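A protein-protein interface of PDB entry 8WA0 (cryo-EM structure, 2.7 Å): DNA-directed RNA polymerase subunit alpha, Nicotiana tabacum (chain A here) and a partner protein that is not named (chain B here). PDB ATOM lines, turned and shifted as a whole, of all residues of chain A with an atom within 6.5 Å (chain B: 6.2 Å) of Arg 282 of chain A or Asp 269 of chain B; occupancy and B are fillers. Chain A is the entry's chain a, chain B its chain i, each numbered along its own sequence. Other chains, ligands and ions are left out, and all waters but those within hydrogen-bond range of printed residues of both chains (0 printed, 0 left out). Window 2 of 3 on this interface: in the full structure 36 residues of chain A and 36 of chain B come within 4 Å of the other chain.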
ATOM      1  N   LEU A 279       3.151 -24.874  23.250  1.00  0.00           N
ATOM      2  CA  LEU A 279       3.139 -23.534  22.739  1.00  0.00           C
ATOM      3  C   LEU A 279       2.484 -23.659  21.412  1.00  0.00           C
ATOM      4  O   LEU A 279       2.350 -24.753  20.898  1.00  0.00           O
ATOM      5  CB  LEU A 279       4.556 -23.080  22.530  1.00  0.00           C
ATOM      6  N   PRO A 280       2.000 -22.547  20.866  1.00  0.00           N
ATOM      7  CA  PRO A 280       1.491 -22.650  19.505  1.00  0.00           C
ATOM      8  C   PRO A 280       2.677 -22.922  18.604  1.00  0.00           C
ATOM      9  O   PRO A 280       3.780 -22.470  18.889  1.00  0.00           O
ATOM     10  CB  PRO A 280       0.929 -21.262  19.230  1.00  0.00           C
ATOM     11  CG  PRO A 280       0.678 -20.668  20.569  1.00  0.00           C
ATOM     12  CD  PRO A 280       1.733 -21.229  21.463  1.00  0.00           C
ATOM     13  N   SER A 281       2.434 -23.612  17.498  1.00  0.00           N
ATOM     14  CA  SER A 281       3.506 -23.998  16.588  1.00  0.00           C
ATOM     15  C   SER A 281       4.341 -22.905  15.986  1.00  0.00           C
ATOM     16  O   SER A 281       5.537 -23.083  15.820  1.00  0.00           O
ATOM     17  CB  SER A 281       2.932 -24.831  15.454  1.00  0.00           C
ATOM     18  OG  SER A 281       2.474 -26.078  15.940  1.00  0.00           O
ATOM     19  N   ARG A 282       3.742 -21.781  15.638  1.00  0.00           N
ATOM     20  CA  ARG A 282       4.524 -20.769  14.962  1.00  0.00           C
ATOM     21  C   ARG A 282       5.619 -20.358  15.891  1.00  0.00           C
ATOM     22  O   ARG A 282       6.775 -20.242  15.497  1.00  0.00           O
ATOM     23  CB  ARG A 282       3.678 -19.543  14.691  1.00  0.00           C
ATOM     24  CG  ARG A 282       2.360 -19.804  13.994  1.00  0.00           C
ATOM     25  CD  ARG A 282       1.644 -18.484  13.782  1.00  0.00           C
ATOM     26  NE  ARG A 282       2.585 -17.441  13.388  1.00  0.00           N
ATOM     27  CZ  ARG A 282       2.257 -16.169  13.190  1.00  0.00           C
ATOM     28  NH1 ARG A 282       1.001 -15.774  13.347  1.00  0.00           N
ATOM     29  NH2 ARG A 282       3.184 -15.291  12.833  1.00  0.00           N
ATOM     30  N   ILE A 283       5.258 -20.156  17.144  1.00  0.00           N
ATOM     31  CA  ILE A 283       6.238 -19.759  18.120  1.00  0.00           C
ATOM     32  C   ILE A 283       7.260 -20.856  18.315  1.00  0.00           C
ATOM     33  O   ILE A 283       8.459 -20.592  18.328  1.00  0.00           O
ATOM     34  CB  ILE A 283       5.562 -19.399  19.452  1.00  0.00           C
ATOM     35  CG1 ILE A 283       4.734 -18.126  19.302  1.00  0.00           C
ATOM     36  CG2 ILE A 283       6.594 -19.166  20.536  1.00  0.00           C
ATOM     37  CD1 ILE A 283       3.289 -18.346  18.916  1.00  0.00           C
ATOM     38  N   TYR A 284       6.809 -22.100  18.395  1.00  0.00           N
ATOM     39  CA  TYR A 284       7.739 -23.180  18.677  1.00  0.00           C
ATOM     40  C   TYR A 284       8.768 -23.305  17.599  1.00  0.00           C
ATOM     41  O   TYR A 284       9.951 -23.437  17.877  1.00  0.00           O
ATOM     42  CB  TYR A 284       6.987 -24.497  18.796  1.00  0.00           C
ATOM     43  CG  TYR A 284       7.858 -25.729  18.903  1.00  0.00           C
ATOM     44  CD1 TYR A 284       8.355 -26.147  20.125  1.00  0.00           C
ATOM     45  CD2 TYR A 284       8.162 -26.486  17.783  1.00  0.00           C
ATOM     46  CE1 TYR A 284       9.144 -27.274  20.223  1.00  0.00           C
ATOM     47  CE2 TYR A 284       8.954 -27.608  17.871  1.00  0.00           C
ATOM     48  CZ  TYR A 284       9.436 -28.000  19.094  1.00  0.00           C
ATOM     49  OH  TYR A 284      10.217 -29.121  19.175  1.00  0.00           O
ATOM     50  N   ASN A 285       8.337 -23.236  16.357  1.00  0.00           N
ATOM     51  CA  ASN A 285       9.278 -23.446  15.289  1.00  0.00           C
ATOM     52  C   ASN A 285      10.332 -22.369  15.299  1.00  0.00           C
ATOM     53  O   ASN A 285      11.518 -22.649  15.185  1.00  0.00           O
ATOM     54  CB  ASN A 285       8.555 -23.455  13.953  1.00  0.00           C
ATOM     55  CG  ASN A 285       7.777 -24.728  13.712  1.00  0.00           C
ATOM     56  OD1 ASN A 285       7.050 -24.840  12.728  1.00  0.00           O
ATOM     57  ND2 ASN A 285       7.931 -25.695  14.599  1.00  0.00           N
ATOM     58  N   CYS A 286       9.911 -21.134  15.477  1.00  0.00           N
ATOM     59  CA  CYS A 286      10.858 -20.043  15.428  1.00  0.00           C
ATOM     60  C   CYS A 286      11.868 -20.142  16.541  1.00  0.00           C
ATOM     61  O   CYS A 286      13.055 -19.898  16.340  1.00  0.00           O
ATOM     62  CB  CYS A 286      10.132 -18.709  15.486  1.00  0.00           C
ATOM     63  SG  CYS A 286       9.178 -18.327  14.003  1.00  0.00           S
ATOM     64  N   LEU A 287      11.407 -20.510  17.721  1.00  0.00           N
ATOM     65  CA  LEU A 287      12.306 -20.596  18.845  1.00  0.00           C
ATOM     66  C   LEU A 287      13.369 -21.635  18.592  1.00  0.00           C
ATOM     67  O   LEU A 287      14.540 -21.402  18.851  1.00  0.00           O
ATOM     68  CB  LEU A 287      11.535 -20.987  20.095  1.00  0.00           C
ATOM     69  CG  LEU A 287      10.632 -19.950  20.748  1.00  0.00           C
ATOM     70  CD1 LEU A 287       9.793 -20.620  21.820  1.00  0.00           C
ATOM     71  CD2 LEU A 287      11.460 -18.822  21.335  1.00  0.00           C
ATOM     72  N   HIS A 311      10.262 -12.673  12.588  1.00  0.00           N
ATOM     73  CA  HIS A 311       8.870 -13.108  12.560  1.00  0.00           C
ATOM     74  C   HIS A 311       8.322 -13.376  13.953  1.00  0.00           C
ATOM     75  O   HIS A 311       7.432 -14.206  14.130  1.00  0.00           O
ATOM     76  CB  HIS A 311       8.659 -14.294  11.604  1.00  0.00           C
ATOM     77  CG  HIS A 311       9.289 -14.109  10.259  1.00  0.00           C
ATOM     78  ND1 HIS A 311       8.683 -13.405   9.243  1.00  0.00           N
ATOM     79  CD2 HIS A 311      10.469 -14.546   9.761  1.00  0.00           C
ATOM     80  CE1 HIS A 311       9.463 -13.411   8.178  1.00  0.00           C
ATOM     81  NE2 HIS A 311      10.555 -14.095   8.467  1.00  0.00           N
ATOM     82  N   ARG A 313       6.271 -11.656  17.060  1.00  0.00           N
ATOM     83  CA  ARG A 313       5.406 -10.501  17.342  1.00  0.00           C
ATOM     84  C   ARG A 313       5.446  -9.890  18.735  1.00  0.00           C
ATOM     85  O   ARG A 313       6.294 -10.243  19.548  1.00  0.00           O
ATOM     86  CB  ARG A 313       3.967 -10.816  16.983  1.00  0.00           C
ATOM     87  N   GLU B 268      -1.207 -20.795   7.709  1.00  0.00           N
ATOM     88  CA  GLU B 268      -0.099 -20.643   6.771  1.00  0.00           C
ATOM     89  C   GLU B 268       1.125 -20.003   7.400  1.00  0.00           C
ATOM     90  O   GLU B 268       1.526 -18.909   7.013  1.00  0.00           O
ATOM     91  CB  GLU B 268      -0.540 -19.843   5.548  1.00  0.00           C
ATOM     92  CG  GLU B 268      -1.470 -20.602   4.621  1.00  0.00           C
ATOM     93  CD  GLU B 268      -0.769 -21.738   3.905  1.00  0.00           C
ATOM     94  OE1 GLU B 268       0.226 -21.471   3.202  1.00  0.00           O
ATOM     95  OE2 GLU B 268      -1.219 -22.893   4.036  1.00  0.00           O
ATOM     96  N   ASP B 269       1.734 -20.691   8.354  1.00  0.00           N
ATOM     97  CA  ASP B 269       2.942 -20.184   8.993  1.00  0.00           C
ATOM     98  C   ASP B 269       4.112 -20.805   8.289  1.00  0.00           C
ATOM     99  O   ASP B 269       5.252 -20.664   8.715  1.00  0.00           O
ATOM    100  CB  ASP B 269       2.965 -20.552  10.473  1.00  0.00           C
ATOM    101  CG  ASP B 269       2.959 -22.055  10.712  1.00  0.00           C
ATOM    102  OD1 ASP B 269       2.272 -22.792   9.974  1.00  0.00           O
ATOM    103  OD2 ASP B 269       3.637 -22.500  11.662  1.00  0.00           O
ATOM    104  N   ILE B 270       3.840 -21.470   7.183  1.00  0.00           N
ATOM    105  CA  ILE B 270       4.882 -22.205   6.507  1.00  0.00           C
ATOM    106  C   ILE B 270       6.064 -21.381   6.061  1.00  0.00           C
ATOM    107  O   ILE B 270       7.210 -21.760   6.296  1.00  0.00           O
ATOM    108  CB  ILE B 270       4.254 -22.899   5.277  1.00  0.00           C
ATOM    109  N   SER B 271       5.812 -20.228   5.472  1.00  0.00           N
ATOM    110  CA  SER B 271       6.910 -19.465   4.940  1.00  0.00           C
ATOM    111  C   SER B 271       7.791 -19.088   6.076  1.00  0.00           C
ATOM    112  O   SER B 271       9.008 -19.213   6.005  1.00  0.00           O
ATOM    113  CB  SER B 271       6.372 -18.199   4.303  1.00  0.00           C
ATOM    114  OG  SER B 271       5.311 -18.499   3.415  1.00  0.00           O
ATOM    115  N   PHE B 272       7.171 -18.627   7.144  1.00  0.00           N
ATOM    116  CA  PHE B 272       7.944 -18.184   8.279  1.00  0.00           C
ATOM    117  C   PHE B 272       8.687 -19.283   9.004  1.00  0.00           C
ATOM    118  O   PHE B 272       9.832 -19.095   9.405  1.00  0.00           O
ATOM    119  CB  PHE B 272       7.055 -17.421   9.264  1.00  0.00           C
ATOM    120  CG  PHE B 272       5.940 -16.669   8.612  1.00  0.00           C
ATOM    121  CD1 PHE B 272       6.203 -15.604   7.771  1.00  0.00           C
ATOM    122  CD2 PHE B 272       4.627 -17.024   8.848  1.00  0.00           C
ATOM    123  CE1 PHE B 272       5.172 -14.912   7.167  1.00  0.00           C
ATOM    124  CE2 PHE B 272       3.592 -16.337   8.252  1.00  0.00           C
ATOM    125  CZ  PHE B 272       3.864 -15.278   7.410  1.00  0.00           C
ATOM    126  N   SER B 273       8.061 -20.438   9.178  1.00  0.00           N
ATOM    127  CA  SER B 273       8.697 -21.439  10.019  1.00  0.00           C
ATOM    128  C   SER B 273       9.111 -22.807   9.523  1.00  0.00           C
ATOM    129  O   SER B 273       9.719 -23.561  10.273  1.00  0.00           O
ATOM    130  CB  SER B 273       7.783 -21.652  11.211  1.00  0.00           C
ATOM    131  OG  SER B 273       6.570 -22.262  10.811  1.00  0.00           O
ATOM    132  N   TYR B 274       8.877 -23.150   8.273  1.00  0.00           N
ATOM    133  CA  TYR B 274       9.199 -24.520   7.879  1.00  0.00           C
ATOM    134  C   TYR B 274      10.688 -24.938   7.894  1.00  0.00           C
ATOM    135  O   TYR B 274      11.036 -25.868   8.608  1.00  0.00           O
ATOM    136  CB  TYR B 274       8.434 -24.940   6.626  1.00  0.00           C
ATOM    137  CG  TYR B 274       6.995 -25.315   6.922  1.00  0.00           C
ATOM    138  CD1 TYR B 274       6.403 -24.975   8.131  1.00  0.00           C
ATOM    139  CD2 TYR B 274       6.235 -26.014   6.001  1.00  0.00           C
ATOM    140  CE1 TYR B 274       5.096 -25.308   8.410  1.00  0.00           C
ATOM    141  CE2 TYR B 274       4.923 -26.352   6.271  1.00  0.00           C
ATOM    142  CZ  TYR B 274       4.361 -25.995   7.476  1.00  0.00           C
ATOM    143  OH  TYR B 274       3.059 -26.333   7.754  1.00  0.00           O
ATOM    144  N   ARG B 368       7.229 -32.828  20.461  1.00  0.00           N
ATOM    145  CA  ARG B 368       5.972 -32.130  20.584  1.00  0.00           C
ATOM    146  C   ARG B 368       4.807 -32.988  20.245  1.00  0.00           C
ATOM    147  O   ARG B 368       3.770 -32.886  20.879  1.00  0.00           O
ATOM    148  CB  ARG B 368       5.985 -30.866  19.781  1.00  0.00           C
ATOM    149  CG  ARG B 368       6.412 -30.973  18.345  1.00  0.00           C
ATOM    150  CD  ARG B 368       6.126 -29.650  17.668  1.00  0.00           C
ATOM    151  NE  ARG B 368       6.443 -29.703  16.255  1.00  0.00           N
ATOM    152  CZ  ARG B 368       6.133 -28.757  15.386  1.00  0.00           C
ATOM    153  NH1 ARG B 368       5.497 -27.667  15.784  1.00  0.00           N
ATOM    154  NH2 ARG B 368       6.456 -28.906  14.118  1.00  0.00           N
ATOM    155  N   ASP B 412      -0.860 -30.387  12.854  1.00  0.00           N
ATOM    156  CA  ASP B 412       0.151 -29.445  12.397  1.00  0.00           C
ATOM    157  C   ASP B 412       1.461 -30.112  12.019  1.00  0.00           C
ATOM    158  O   ASP B 412       2.066 -29.767  11.011  1.00  0.00           O
ATOM    159  CB  ASP B 412       0.408 -28.395  13.457  1.00  0.00           C
ATOM    160  CG  ASP B 412       1.183 -27.215  12.918  1.00  0.00           C
ATOM    161  OD1 ASP B 412       0.560 -26.336  12.290  1.00  0.00           O
ATOM    162  OD2 ASP B 412       2.417 -27.172  13.105  1.00  0.00           O
ATOM    163  N   LYS B 415       1.001 -31.671   8.756  1.00  0.00           N
ATOM    164  CA  LYS B 415       0.996 -30.699   7.688  1.00  0.00           C
ATOM    165  C   LYS B 415       2.382 -30.290   7.226  1.00  0.00           C
ATOM    166  O   LYS B 415       2.619 -30.176   6.029  1.00  0.00           O
ATOM    167  CB  LYS B 415       0.234 -29.467   8.155  1.00  0.00           C
ATOM    168  CG  LYS B 415      -0.011 -28.413   7.097  1.00  0.00           C
ATOM    169  CD  LYS B 415      -0.477 -27.132   7.765  1.00  0.00           C
ATOM    170  CE  LYS B 415      -1.451 -27.441   8.891  1.00  0.00           C
ATOM    171  NZ  LYS B 415      -1.817 -26.222   9.661  1.00  0.00           N
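Of chain B, only Asp 269 comes within 4 Å of Arg 282 of chain A. Of the printed residues of chain B, Tyr 284 of chain A touches Arg 368 (3.5 Å). Printed residues of chain A within 4 Å of Ser 273 of chain B: Asn 285. Of the printed residues of chain A, Arg 368 of chain B touches Ser 281, Tyr 284 and Asn 285.
The guanidinium group (NH1) of Arg 368 of chain B lies close to the side-chain amide nitrogen (ND2) of Asn 285 of chain A (3.3 Å). The side-chain amide oxygen (OD1) of Asn 285 of chain A sits at hydrogen-bond distance from the side-chain hydroxyl (OG) of Ser 273 of chain B, 3.2 Å away. The side-chain hydroxyl (OG) of Ser 281 of chain A lies within hydrogen-bond range of the guanidinium group (NH1) of Arg 368 of chain B (3.4 Å). The side-chain hydroxyl of Ser 281 of chain A lies within hydrogen-bond range of the side-chain carboxylate of Asp 412 of chain B (3.0 Å).
Among the printed residues, merely in contact across the chains: Tyr 284 of chain A with Arg 368 of chain B, His 311 of chain A with Phe 272 of chain B and Arg 282 of chain A with Asp 269 of chain B.
Hydrophobic or aromatic side chains of chain A within 4 Å of the printed part of chain B: Tyr 284 and His 311. Hydrophobic or aromatic side chains of chain B that line the printed part of chain A: Phe 272. Among the printed residues, 7 pairs touch across the chains. Among the printed residues, no Asp or Glu carboxylate lies within 4 Å of a Lys or Arg side-chain nitrogen of the other chain.
The side-chain carboxylate (OD1) of Asp 412 of chain B lies within salt-bridge range of the side-chain amino group (NZ) of Lys 415 of chain B (3.5 Å). The backbone carbonyl oxygen (O) of Asp 269 of chain B sits at hydrogen-bond distance from the side-chain hydroxyl (OG) of Ser 273 of chain B. The backbone carbonyl oxygen (O) of Arg 282 of chain A lies within hydrogen-bond range of the side-chain sulfur (SG) of Cys 286 of chain A (3.4 Å).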
